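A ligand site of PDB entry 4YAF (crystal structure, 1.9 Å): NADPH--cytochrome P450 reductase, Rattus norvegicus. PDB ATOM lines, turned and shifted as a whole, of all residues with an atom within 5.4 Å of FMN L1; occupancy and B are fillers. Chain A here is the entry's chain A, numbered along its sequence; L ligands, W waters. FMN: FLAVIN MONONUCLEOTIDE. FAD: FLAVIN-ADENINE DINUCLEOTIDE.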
ATOM      1  N   GLY A  29      -7.243  12.886  17.189  1.00  0.00           N
ATOM      2  CA  GLY A  29      -6.327  13.811  16.540  1.00  0.00           C
ATOM      3  C   GLY A  29      -7.208  14.635  15.642  1.00  0.00           C
ATOM      4  O   GLY A  29      -7.735  14.146  14.642  1.00  0.00           O
ATOM      5  N   SER A  30      -7.376  15.906  15.992  1.00  0.00           N
ATOM      6  CA  SER A  30      -8.313  16.765  15.287  1.00  0.00           C
ATOM      7  C   SER A  30      -7.829  18.197  15.189  1.00  0.00           C
ATOM      8  O   SER A  30      -7.034  18.658  16.007  1.00  0.00           O
ATOM      9  CB  SER A  30      -9.687  16.718  15.963  1.00  0.00           C
ATOM     10  OG  SER A  30     -10.666  17.369  15.174  1.00  0.00           O
ATOM     11  N   GLN A  31      -8.338  18.895  14.175  1.00  0.00           N
ATOM     12  CA  GLN A  31      -8.062  20.325  14.005  1.00  0.00           C
ATOM     13  C   GLN A  31      -9.366  21.065  13.701  1.00  0.00           C
ATOM     14  O   GLN A  31      -9.571  22.178  14.164  1.00  0.00           O
ATOM     15  CB  GLN A  31      -7.046  20.560  12.876  1.00  0.00           C
ATOM     16  CG  GLN A  31      -5.665  20.007  13.192  1.00  0.00           C
ATOM     17  CD  GLN A  31      -4.571  20.541  12.280  1.00  0.00           C
ATOM     18  OE1 GLN A  31      -3.423  20.086  12.329  1.00  0.00           O
ATOM     19  NE2 GLN A  31      -4.915  21.524  11.446  1.00  0.00           N
ATOM     20  N   THR A  32     -10.243  20.430  12.941  1.00  0.00           N
ATOM     21  CA  THR A  32     -11.530  21.039  12.594  1.00  0.00           C
ATOM     22  C   THR A  32     -12.677  20.404  13.395  1.00  0.00           C
ATOM     23  O   THR A  32     -13.851  20.674  13.119  1.00  0.00           O
ATOM     24  CB  THR A  32     -11.818  20.895  11.089  1.00  0.00           C
ATOM     25  OG1 THR A  32     -10.645  21.243  10.342  1.00  0.00           O
ATOM     26  CG2 THR A  32     -12.944  21.815  10.679  1.00  0.00           C
ATOM     27  N   GLY A  33     -12.332  19.570  14.361  1.00  0.00           N
ATOM     28  CA  GLY A  33     -13.344  18.949  15.211  1.00  0.00           C
ATOM     29  C   GLY A  33     -14.053  17.680  14.756  1.00  0.00           C
ATOM     30  O   GLY A  33     -14.880  17.149  15.503  1.00  0.00           O
ATOM     31  N   THR A  34     -13.751  17.189  13.563  1.00  0.00           N
ATOM     32  CA  THR A  34     -14.400  15.993  13.048  1.00  0.00           C
ATOM     33  C   THR A  34     -14.020  14.729  13.825  1.00  0.00           C
ATOM     34  O   THR A  34     -14.900  13.944  14.211  1.00  0.00           O
ATOM     35  CB  THR A  34     -14.056  15.761  11.554  1.00  0.00           C
ATOM     36  OG1 THR A  34     -14.387  16.940  10.807  1.00  0.00           O
ATOM     37  CG2 THR A  34     -14.851  14.580  11.000  1.00  0.00           C
ATOM     38  N   ALA A  35     -12.724  14.526  14.047  1.00  0.00           N
ATOM     39  CA  ALA A  35     -12.244  13.359  14.779  1.00  0.00           C
ATOM     40  C   ALA A  35     -12.641  13.444  16.237  1.00  0.00           C
ATOM     41  O   ALA A  35     -12.905  12.422  16.885  1.00  0.00           O
ATOM     42  CB  ALA A  35     -10.716  13.248  14.653  1.00  0.00           C
ATOM     43  N   GLU A  36     -12.676  14.656  16.770  1.00  0.00           N
ATOM     44  CA  GLU A  36     -13.070  14.867  18.149  1.00  0.00           C
ATOM     45  C   GLU A  36     -14.511  14.426  18.321  1.00  0.00           C
ATOM     46  O   GLU A  36     -14.876  13.816  19.315  1.00  0.00           O
ATOM     47  CB  GLU A  36     -12.918  16.347  18.529  1.00  0.00           C
ATOM     48  CG  GLU A  36     -13.314  16.652  19.963  1.00  0.00           C
ATOM     49  CD  GLU A  36     -12.996  18.086  20.361  1.00  0.00           C
ATOM     50  OE1 GLU A  36     -11.816  18.491  20.284  1.00  0.00           O
ATOM     51  OE2 GLU A  36     -13.934  18.813  20.751  1.00  0.00           O
ATOM     52  N   ALA A  82      -7.017  12.305  12.347  1.00  0.00           N
ATOM     53  CA  ALA A  82      -7.086  12.953  11.047  1.00  0.00           C
ATOM     54  C   ALA A  82      -5.661  13.268  10.593  1.00  0.00           C
ATOM     55  O   ALA A  82      -4.747  13.367  11.422  1.00  0.00           O
ATOM     56  CB  ALA A  82      -7.914  14.235  11.122  1.00  0.00           C
ATOM     57  N   THR A  83      -5.492  13.443   9.290  1.00  0.00           N
ATOM     58  CA  THR A  83      -4.190  13.750   8.696  1.00  0.00           C
ATOM     59  C   THR A  83      -4.202  15.155   8.109  1.00  0.00           C
ATOM     60  O   THR A  83      -5.230  15.616   7.617  1.00  0.00           O
ATOM     61  CB  THR A  83      -3.845  12.763   7.559  1.00  0.00           C
ATOM     62  OG1 THR A  83      -3.764  11.432   8.085  1.00  0.00           O
ATOM     63  CG2 THR A  83      -2.523  13.140   6.919  1.00  0.00           C
ATOM     64  N   TYR A  84      -3.061  15.835   8.170  1.00  0.00           N
ATOM     65  CA  TYR A  84      -2.954  17.170   7.607  1.00  0.00           C
ATOM     66  C   TYR A  84      -1.873  17.162   6.538  1.00  0.00           C
ATOM     67  O   TYR A  84      -1.308  16.117   6.220  1.00  0.00           O
ATOM     68  CB  TYR A  84      -3.057  18.235   8.708  1.00  0.00           C
ATOM     69  CG  TYR A  84      -4.492  18.577   9.054  1.00  0.00           C
ATOM     70  CD1 TYR A  84      -5.259  17.723   9.856  1.00  0.00           C
ATOM     71  CD2 TYR A  84      -5.091  19.727   8.553  1.00  0.00           C
ATOM     72  CE1 TYR A  84      -6.596  18.019  10.135  1.00  0.00           C
ATOM     73  CE2 TYR A  84      -6.419  20.034   8.831  1.00  0.00           C
ATOM     74  CZ  TYR A  84      -7.166  19.170   9.612  1.00  0.00           C
ATOM     75  OH  TYR A  84      -8.485  19.488   9.889  1.00  0.00           O
ATOM     76  N   GLY A  85      -1.624  18.338   5.973  1.00  0.00           N
ATOM     77  CA  GLY A  85      -0.627  18.536   4.929  1.00  0.00           C
ATOM     78  C   GLY A  85       0.631  17.687   4.971  1.00  0.00           C
ATOM     79  O   GLY A  85       1.383  17.711   5.940  1.00  0.00           O
ATOM     80  N   GLU A  86       0.872  16.946   3.889  1.00  0.00           N
ATOM     81  CA  GLU A  86       2.056  16.094   3.778  1.00  0.00           C
ATOM     82  C   GLU A  86       2.034  14.885   4.707  1.00  0.00           C
ATOM     83  O   GLU A  86       3.088  14.413   5.147  1.00  0.00           O
ATOM     84  CB  GLU A  86       3.334  16.905   4.020  1.00  0.00           C
ATOM     85  CG  GLU A  86       3.639  17.928   2.936  1.00  0.00           C
ATOM     86  CD  GLU A  86       4.840  18.798   3.261  1.00  0.00           C
ATOM     87  OE1 GLU A  86       4.742  19.624   4.205  1.00  0.00           O
ATOM     88  OE2 GLU A  86       5.889  18.648   2.596  1.00  0.00           O
ATOM     89  N   GLY A  87       0.840  14.390   5.002  1.00  0.00           N
ATOM     90  CA  GLY A  87       0.718  13.231   5.877  1.00  0.00           C
ATOM     91  C   GLY A  87       1.204  13.437   7.290  1.00  0.00           C
ATOM     92  O   GLY A  87       1.745  12.510   7.903  1.00  0.00           O
ATOM     93  N   ASP A  88       1.028  14.646   7.816  1.00  0.00           N
ATOM     94  CA  ASP A  88       1.452  14.946   9.189  1.00  0.00           C
ATOM     95  C   ASP A  88       0.292  14.811  10.153  1.00  0.00           C
ATOM     96  O   ASP A  88      -0.874  14.824   9.750  1.00  0.00           O
ATOM     97  CB  ASP A  88       2.025  16.364   9.275  1.00  0.00           C
ATOM     98  CG  ASP A  88       3.287  16.535   8.461  1.00  0.00           C
ATOM     99  OD1 ASP A  88       4.219  15.726   8.610  1.00  0.00           O
ATOM    100  OD2 ASP A  88       3.330  17.501   7.664  1.00  0.00           O
ATOM    101  N   THR A  90      -2.284  15.912  13.307  1.00  0.00           N
ATOM    102  CA  THR A  90      -2.946  17.170  13.630  1.00  0.00           C
ATOM    103  C   THR A  90      -2.024  17.804  14.668  1.00  0.00           C
ATOM    104  O   THR A  90      -1.264  17.099  15.338  1.00  0.00           O
ATOM    105  CB  THR A  90      -4.333  16.948  14.247  1.00  0.00           C
ATOM    106  OG1 THR A  90      -4.222  16.052  15.357  1.00  0.00           O
ATOM    107  CG2 THR A  90      -5.299  16.371  13.219  1.00  0.00           C
ATOM    108  N   LEU A 117      -9.096   9.546   9.628  1.00  0.00           N
ATOM    109  CA  LEU A 117      -9.867  10.527   8.861  1.00  0.00           C
ATOM    110  C   LEU A 117      -8.911  11.155   7.855  1.00  0.00           C
ATOM    111  O   LEU A 117      -7.893  11.742   8.244  1.00  0.00           O
ATOM    112  CB  LEU A 117     -10.414  11.635   9.767  1.00  0.00           C
ATOM    113  CG  LEU A 117     -11.471  11.313  10.824  1.00  0.00           C
ATOM    114  CD1 LEU A 117     -10.825  10.647  12.035  1.00  0.00           C
ATOM    115  CD2 LEU A 117     -12.147  12.606  11.247  1.00  0.00           C
ATOM    116  N   GLY A 118      -9.229  11.020   6.574  1.00  0.00           N
ATOM    117  CA  GLY A 118      -8.379  11.579   5.551  1.00  0.00           C
ATOM    118  C   GLY A 118      -9.200  12.071   4.376  1.00  0.00           C
ATOM    119  O   GLY A 118     -10.388  12.362   4.512  1.00  0.00           O
ATOM    120  N   ASN A 119      -8.558  12.163   3.218  1.00  0.00           N
ATOM    121  CA  ASN A 119      -9.208  12.607   1.991  1.00  0.00           C
ATOM    122  C   ASN A 119      -8.352  12.132   0.819  1.00  0.00           C
ATOM    123  O   ASN A 119      -7.197  12.543   0.694  1.00  0.00           O
ATOM    124  CB  ASN A 119      -9.328  14.133   1.980  1.00  0.00           C
ATOM    125  CG  ASN A 119     -10.120  14.638   0.791  1.00  0.00           C
ATOM    126  OD1 ASN A 119      -9.918  14.192  -0.346  1.00  0.00           O
ATOM    127  ND2 ASN A 119     -11.018  15.581   1.033  1.00  0.00           N
ATOM    128  N   LYS A 120      -8.919  11.287  -0.036  1.00  0.00           N
ATOM    129  CA  LYS A 120      -8.204  10.732  -1.171  1.00  0.00           C
ATOM    130  C   LYS A 120      -7.609  11.722  -2.187  1.00  0.00           C
ATOM    131  O   LYS A 120      -6.819  11.320  -3.036  1.00  0.00           O
ATOM    132  CB  LYS A 120      -9.082   9.735  -1.929  1.00  0.00           C
ATOM    133  CG  LYS A 120      -9.288   8.399  -1.237  1.00  0.00           C
ATOM    134  CD  LYS A 120      -9.872   7.384  -2.211  1.00  0.00           C
ATOM    135  CE  LYS A 120     -10.120   6.032  -1.554  1.00  0.00           C
ATOM    136  NZ  LYS A 120     -11.223   6.094  -0.567  1.00  0.00           N
ATOM    137  N   TYR A 122      -5.489  13.746  -1.629  1.00  0.00           N
ATOM    138  CA  TYR A 122      -4.152  14.082  -1.152  1.00  0.00           C
ATOM    139  C   TYR A 122      -3.147  12.958  -1.363  1.00  0.00           C
ATOM    140  O   TYR A 122      -3.519  11.786  -1.471  1.00  0.00           O
ATOM    141  CB  TYR A 122      -4.187  14.470   0.326  1.00  0.00           C
ATOM    142  CG  TYR A 122      -4.962  15.728   0.629  1.00  0.00           C
ATOM    143  CD1 TYR A 122      -6.356  15.717   0.690  1.00  0.00           C
ATOM    144  CD2 TYR A 122      -4.309  16.930   0.861  1.00  0.00           C
ATOM    145  CE1 TYR A 122      -7.073  16.869   0.985  1.00  0.00           C
ATOM    146  CE2 TYR A 122      -5.017  18.093   1.154  1.00  0.00           C
ATOM    147  CZ  TYR A 122      -6.398  18.052   1.216  1.00  0.00           C
ATOM    148  OH  TYR A 122      -7.094  19.207   1.529  1.00  0.00           O
ATOM    149  N   HIS A 124      -0.599  11.814   0.738  1.00  0.00           N
ATOM    150  CA  HIS A 124      -0.556  10.934   1.893  1.00  0.00           C
ATOM    151  C   HIS A 124      -1.935  10.753   2.517  1.00  0.00           C
ATOM    152  O   HIS A 124      -2.251  11.355   3.544  1.00  0.00           O
ATOM    153  CB  HIS A 124       0.421  11.492   2.921  1.00  0.00           C
ATOM    154  CG  HIS A 124       1.749  11.872   2.350  1.00  0.00           C
ATOM    155  ND1 HIS A 124       1.945  13.025   1.610  1.00  0.00           N
ATOM    156  CD2 HIS A 124       2.960  11.251   2.393  1.00  0.00           C
ATOM    157  CE1 HIS A 124       3.203  13.098   1.224  1.00  0.00           C
ATOM    158  NE2 HIS A 124       3.842  12.030   1.686  1.00  0.00           N
ATOM    159  N   PHE A 125      -2.753   9.909   1.895  1.00  0.00           N
ATOM    160  CA  PHE A 125      -4.109   9.630   2.351  1.00  0.00           C
ATOM    161  C   PHE A 125      -4.129   8.845   3.668  1.00  0.00           C
ATOM    162  O   PHE A 125      -3.662   7.701   3.726  1.00  0.00           O
ATOM    163  CB  PHE A 125      -4.863   8.858   1.277  1.00  0.00           C
ATOM    164  CG  PHE A 125      -6.217   8.387   1.705  1.00  0.00           C
ATOM    165  CD1 PHE A 125      -7.198   9.292   2.107  1.00  0.00           C
ATOM    166  CD2 PHE A 125      -6.525   7.025   1.703  1.00  0.00           C
ATOM    167  CE1 PHE A 125      -8.456   8.848   2.505  1.00  0.00           C
ATOM    168  CE2 PHE A 125      -7.783   6.581   2.101  1.00  0.00           C
ATOM    169  CZ  PHE A 125      -8.753   7.487   2.503  1.00  0.00           C
ATOM    170  N   ASN A 126      -4.686   9.457   4.705  1.00  0.00           N
ATOM    171  CA  ASN A 126      -4.788   8.836   6.028  1.00  0.00           C
ATOM    172  C   ASN A 126      -3.445   8.351   6.544  1.00  0.00           C
ATOM    173  O   ASN A 126      -3.364   7.308   7.204  1.00  0.00           O
ATOM    174  CB  ASN A 126      -5.768   7.658   5.994  1.00  0.00           C
ATOM    175  CG  ASN A 126      -7.187   8.062   6.344  1.00  0.00           C
ATOM    176  OD1 ASN A 126      -7.430   8.670   7.394  1.00  0.00           O
ATOM    177  ND2 ASN A 126      -8.138   7.736   5.471  1.00  0.00           N
ATOM    178  N   ALA A 127      -2.391   9.106   6.256  1.00  0.00           N
ATOM    179  CA  ALA A 127      -1.054   8.738   6.695  1.00  0.00           C
ATOM    180  C   ALA A 127      -0.964   8.595   8.214  1.00  0.00           C
ATOM    181  O   ALA A 127      -0.341   7.648   8.710  1.00  0.00           O
ATOM    182  CB  ALA A 127      -0.041   9.780   6.212  1.00  0.00           C
ATOM    183  N   ASP A 152     -12.973  11.881   3.267  1.00  0.00           N
ATOM    184  CA  ASP A 152     -13.806  13.076   3.207  1.00  0.00           C
ATOM    185  C   ASP A 152     -14.152  13.503   1.773  1.00  0.00           C
ATOM    186  O   ASP A 152     -14.909  14.455   1.580  1.00  0.00           O
ATOM    187  CB  ASP A 152     -13.121  14.217   3.963  1.00  0.00           C
ATOM    188  CG  ASP A 152     -14.083  15.306   4.383  1.00  0.00           C
ATOM    189  OD1 ASP A 152     -15.191  14.969   4.872  1.00  0.00           O
ATOM    190  OD2 ASP A 152     -13.747  16.501   4.232  1.00  0.00           O
ATOM    191  N   LEU A 156     -17.393  10.802   4.571  1.00  0.00           N
ATOM    192  CA  LEU A 156     -16.745  10.399   5.797  1.00  0.00           C
ATOM    193  C   LEU A 156     -17.717   9.893   6.857  1.00  0.00           C
ATOM    194  O   LEU A 156     -17.449   8.905   7.517  1.00  0.00           O
ATOM    195  CB  LEU A 156     -15.930  11.571   6.349  1.00  0.00           C
ATOM    196  CG  LEU A 156     -15.146  11.312   7.644  1.00  0.00           C
ATOM    197  CD1 LEU A 156     -14.235  10.111   7.446  1.00  0.00           C
ATOM    198  CD2 LEU A 156     -14.343  12.554   8.012  1.00  0.00           C
ATOM    199  N   VAL A 620      -3.393  24.090  -1.210  1.00  0.00           N
ATOM    200  CA  VAL A 620      -4.663  23.829  -1.878  1.00  0.00           C
ATOM    201  C   VAL A 620      -5.754  23.480  -0.888  1.00  0.00           C
ATOM    202  O   VAL A 620      -5.493  22.967   0.207  1.00  0.00           O
ATOM    203  CB  VAL A 620      -4.497  22.682  -2.909  1.00  0.00           C
ATOM    204  CG1 VAL A 620      -3.634  23.164  -4.069  1.00  0.00           C
ATOM    205  CG2 VAL A 620      -3.868  21.452  -2.256  1.00  0.00           C
HETATM  206  N1  FMN L   1      -6.259  14.142   4.367  1.00  0.00           N
HETATM  207  C2  FMN L   1      -5.348  13.206   4.063  1.00  0.00           C
HETATM  208  O2  FMN L   1      -5.667  12.020   3.971  1.00  0.00           O
HETATM  209  N3  FMN L   1      -4.051  13.634   3.854  1.00  0.00           N
HETATM  210  C4  FMN L   1      -3.584  14.963   3.924  1.00  0.00           C
HETATM  211  O4  FMN L   1      -2.376  15.101   3.700  1.00  0.00           O
HETATM  212  C4A FMN L   1      -4.539  15.965   4.238  1.00  0.00           C
HETATM  213  N5  FMN L   1      -4.093  17.302   4.309  1.00  0.00           N
HETATM  214  C5A FMN L   1      -5.104  18.230   4.613  1.00  0.00           C
HETATM  215  C6  FMN L   1      -4.680  19.605   4.684  1.00  0.00           C
HETATM  216  C7  FMN L   1      -5.590  20.641   4.982  1.00  0.00           C
HETATM  217  C7M FMN L   1      -5.004  22.077   5.005  1.00  0.00           C
HETATM  218  C8  FMN L   1      -7.043  20.334   5.237  1.00  0.00           C
HETATM  219  C8M FMN L   1      -8.025  21.263   5.538  1.00  0.00           C
HETATM  220  C9  FMN L   1      -7.449  19.011   5.182  1.00  0.00           C
HETATM  221  C9A FMN L   1      -6.517  17.926   4.874  1.00  0.00           C
HETATM  222  N10 FMN L   1      -6.887  16.494   4.782  1.00  0.00           N
HETATM  223  C10 FMN L   1      -5.871  15.475   4.454  1.00  0.00           C
HETATM  224  C1' FMN L   1      -8.263  16.071   5.018  1.00  0.00           C
HETATM  225  C2' FMN L   1      -8.601  15.842   6.519  1.00  0.00           C
HETATM  226  O2' FMN L   1      -7.695  14.801   7.067  1.00  0.00           O
HETATM  227  C3' FMN L   1     -10.055  15.419   6.671  1.00  0.00           C
HETATM  228  O3' FMN L   1     -10.863  16.488   6.124  1.00  0.00           O
HETATM  229  C4' FMN L   1     -10.371  15.182   8.191  1.00  0.00           C
HETATM  230  O4' FMN L   1     -11.777  14.781   8.116  1.00  0.00           O
HETATM  231  C5' FMN L   1     -10.349  16.436   9.049  1.00  0.00           C
HETATM  232  O5' FMN L   1     -10.638  16.136  10.480  1.00  0.00           O
HETATM  233  P   FMN L   1     -10.753  17.174  11.644  1.00  0.00           P
HETATM  234  O1P FMN L   1     -11.948  18.028  11.424  1.00  0.00           O
HETATM  235  O2P FMN L   1      -9.335  17.839  11.742  1.00  0.00           O
HETATM  236  O3P FMN L   1     -11.047  16.211  12.894  1.00  0.00           O
HETATM  237  PA  FAD L   2     -18.957  27.738   4.819  1.00  0.00           P
HETATM  238  O1A FAD L   2     -20.166  28.189   5.531  1.00  0.00           O
HETATM  239  O2A FAD L   2     -17.870  27.095   5.588  1.00  0.00           O
HETATM  240  O5B FAD L   2     -19.403  26.754   3.631  1.00  0.00           O
HETATM  241  C5B FAD L   2     -18.433  25.992   2.909  1.00  0.00           C
HETATM  242  C4B FAD L   2     -19.119  24.777   2.298  1.00  0.00           C
HETATM  243  O4B FAD L   2     -20.196  25.164   1.432  1.00  0.00           O
HETATM  244  C3B FAD L   2     -18.194  24.048   1.336  1.00  0.00           C
HETATM  245  O3B FAD L   2     -17.258  23.262   2.097  1.00  0.00           O
HETATM  246  C2B FAD L   2     -19.218  23.126   0.706  1.00  0.00           C
HETATM  247  O2B FAD L   2     -19.526  22.054   1.603  1.00  0.00           O
HETATM  248  C1B FAD L   2     -20.440  24.043   0.566  1.00  0.00           C
HETATM  249  N9A FAD L   2     -20.567  24.583  -0.803  1.00  0.00           N
HETATM  250  C8A FAD L   2     -19.873  25.756  -1.357  1.00  0.00           C
HETATM  251  N7A FAD L   2     -20.444  25.807  -2.708  1.00  0.00           N
HETATM  252  C5A FAD L   2     -21.316  24.814  -2.843  1.00  0.00           C
HETATM  253  C6A FAD L   2     -22.061  24.485  -3.895  1.00  0.00           C
HETATM  254  N6A FAD L   2     -22.040  25.336  -4.924  1.00  0.00           N
HETATM  255  N1A FAD L   2     -22.845  23.405  -3.912  1.00  0.00           N
HETATM  256  C2A FAD L   2     -22.900  22.586  -2.782  1.00  0.00           C
HETATM  257  N3A FAD L   2     -22.093  22.942  -1.697  1.00  0.00           N
HETATM  258  C4A FAD L   2     -21.327  24.047  -1.750  1.00  0.00           C
HETATM  259  N1  FAD L   2     -10.640  30.546   0.689  1.00  0.00           N
HETATM  260  C2  FAD L   2     -10.453  31.772   0.035  1.00  0.00           C
HETATM  261  O2  FAD L   2     -11.376  32.275  -0.599  1.00  0.00           O
HETATM  262  N3  FAD L   2      -9.189  32.380   0.059  1.00  0.00           N
HETATM  263  C4  FAD L   2      -8.114  31.750   0.698  1.00  0.00           C
HETATM  264  O4  FAD L   2      -7.016  32.315   0.739  1.00  0.00           O
HETATM  265  C4X FAD L   2      -8.304  30.532   1.331  1.00  0.00           C
HETATM  266  N5  FAD L   2      -7.260  29.850   1.815  1.00  0.00           N
HETATM  267  C5X FAD L   2      -7.454  28.671   2.436  1.00  0.00           C
HETATM  268  C6  FAD L   2      -6.364  27.997   2.985  1.00  0.00           C
HETATM  269  C7  FAD L   2      -6.562  26.811   3.667  1.00  0.00           C
HETATM  270  C7M FAD L   2      -5.497  26.211   4.335  1.00  0.00           C
HETATM  271  C8  FAD L   2      -7.849  26.279   3.791  1.00  0.00           C
HETATM  272  C8M FAD L   2      -8.056  25.093   4.484  1.00  0.00           C
HETATM  273  C9  FAD L   2      -8.929  26.965   3.250  1.00  0.00           C
HETATM  274  C9A FAD L   2      -8.741  28.161   2.578  1.00  0.00           C
HETATM  275  N10 FAD L   2      -9.786  28.852   2.094  1.00  0.00           N
HETATM  276  C10 FAD L   2      -9.557  29.926   1.326  1.00  0.00           C
HETATM  277  C1' FAD L   2     -11.175  28.374   2.244  1.00  0.00           C
HETATM  278  C2' FAD L   2     -11.797  29.032   3.485  1.00  0.00           C
HETATM  279  O2' FAD L   2     -11.130  28.566   4.652  1.00  0.00           O
HETATM  280  C3' FAD L   2     -13.294  28.744   3.613  1.00  0.00           C
HETATM  281  O3' FAD L   2     -13.537  27.342   3.507  1.00  0.00           O
HETATM  282  C4' FAD L   2     -14.104  29.484   2.542  1.00  0.00           C
HETATM  283  O4' FAD L   2     -13.827  30.886   2.584  1.00  0.00           O
HETATM  284  C5' FAD L   2     -15.604  29.254   2.797  1.00  0.00           C
HETATM  285  O5' FAD L   2     -15.906  29.563   4.162  1.00  0.00           O
HETATM  286  P   FAD L   2     -17.365  30.079   4.610  1.00  0.00           P
HETATM  287  O1P FAD L   2     -17.638  31.367   3.932  1.00  0.00           O
HETATM  288  O2P FAD L   2     -17.439  30.041   6.087  1.00  0.00           O
HETATM  289  O3P FAD L   2     -18.355  28.979   3.978  1.00  0.00           O
HETATM  290  O   HOH W   1      -9.232  21.999   2.551  1.00  0.00           O
HETATM  291  O   HOH W   2     -13.943  16.783   7.942  1.00  0.00           O
HETATM  292  O   HOH W   3      -0.691  14.807   1.620  1.00  0.00           O
HETATM  293  O   HOH W   4      -6.231  23.865   7.638  1.00  0.00           O
HETATM  294  O   HOH W   5     -10.617  19.761   7.191  1.00  0.00           O
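Water W3 lies within hydrogen-bond range of an oxygen (O4) of FMN L1, the backbone NH of His 124 and the backbone NH of Glu 86. Water W2 bridges the side-chain hydroxyl of Thr 34 and an oxygen (O4') of FMN L1. Water W5 lies within hydrogen-bond range of OH of Tyr 84, O3' of FMN L1 and OG1 of Thr 32.
The backbone NH of Gly 33 sits at hydrogen-bond distance from the side-chain hydroxyl of Ser 30, 2.9 Å away. The side-chain hydroxyl (OG) of Ser 30 sits at hydrogen-bond distance from the backbone NH (N) of Thr 34, 3.5 Å away. The backbone NH (N) of Ser 30 sits at hydrogen-bond distance from the side-chain hydroxyl (OG1) of Thr 90, at 3.2 Å. O of Gly 85 sits close to OD2 of Asp 88, 2.6 Å away. OD1 of Asn 126 sits at hydrogen-bond distance from N of Gly 118 (3.1 Å). The side-chain amide oxygen of Asn 126 sits at hydrogen-bond distance from the backbone NH of Leu 117 (2.9 Å). The side-chain hydroxyl (OG1) of Thr 83 sits at hydrogen-bond distance from the backbone NH (N) of Ala 127, at 3.3 Å. The backbone carbonyl oxygen of Gly 29 sits at hydrogen-bond distance from the backbone NH of Ala 82.
CB of Ala 82 touches O5' of FMN L1, 3.4 Å away. N of Glu 86 touches O4 of FMN L1 (3.7 Å). N of Gly 87 touches O4 of FMN L1 (3.5 Å). Gly 118 touches FMN L1 (CA to O2, 3.2 Å). Tyr 122 touches FMN L1. CA of Phe 125 touches O2 of FMN L1, at 3.3 Å. Leu 156 touches FMN L1. Hydrophobic or aromatic side chains within 4 Å of FMN L1: Ala 35, Ala 82, Tyr 84, Leu 117, Tyr 122, Phe 125 and Leu 156. The nearest printed residue that does not touch FMN L1 is Gly 29 (4.3 Å).
OH of Tyr 84 sits at hydrogen-bond distance from O2P of FMN L1 (2.6 Å). A nitrogen (N3) of FMN L1 lies within hydrogen-bond range of the backbone carbonyl oxygen (O) of His 124, at 2.9 Å. A nitrogen (N5) of FMN L1 sits at hydrogen-bond distance from the backbone NH of Gly 85. The backbone NH (N) of Thr 32 sits at hydrogen-bond distance from an oxygen (O2P) of FMN L1, 3.0 Å away. An oxygen (O2') of FMN L1 is in hydrogen-bond range of the backbone carbonyl oxygen of Leu 117 (3.3 Å). An oxygen (O2') of FMN L1 is in hydrogen-bond range of the backbone NH (N) of Thr 83, at 3.4 Å. The backbone NH (N) of Asn 119 is in hydrogen-bond range of an oxygen (O2) of FMN L1. The backbone NH of Ala 35 lies within hydrogen-bond range of an oxygen (O3P) of FMN L1, 2.6 Å away. An oxygen (O2') of FMN L1 is in hydrogen-bond range of the backbone carbonyl oxygen (O) of Thr 83 (2.7 Å). O3P of FMN L1 lies within hydrogen-bond range of OG of Ser 30, 2.6 Å away. N of Thr 34 sits at hydrogen-bond distance from O1P of FMN L1 (2.9 Å). The backbone NH (N) of Gln 31 lies within hydrogen-bond range of an oxygen (O2P) of FMN L1 (2.8 Å). The side-chain carboxylate (OD2) of Asp 152 lies within hydrogen-bond range of an oxygen (O3') of FMN L1. An oxygen (O2) of FMN L1 sits at hydrogen-bond distance from the backbone NH (N) of Asn 126 (2.8 Å). OG1 of Thr 34 is in hydrogen-bond range of O1P of FMN L1. N of Gly 33 sits at hydrogen-bond distance from O1P of FMN L1 (3.3 Å).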
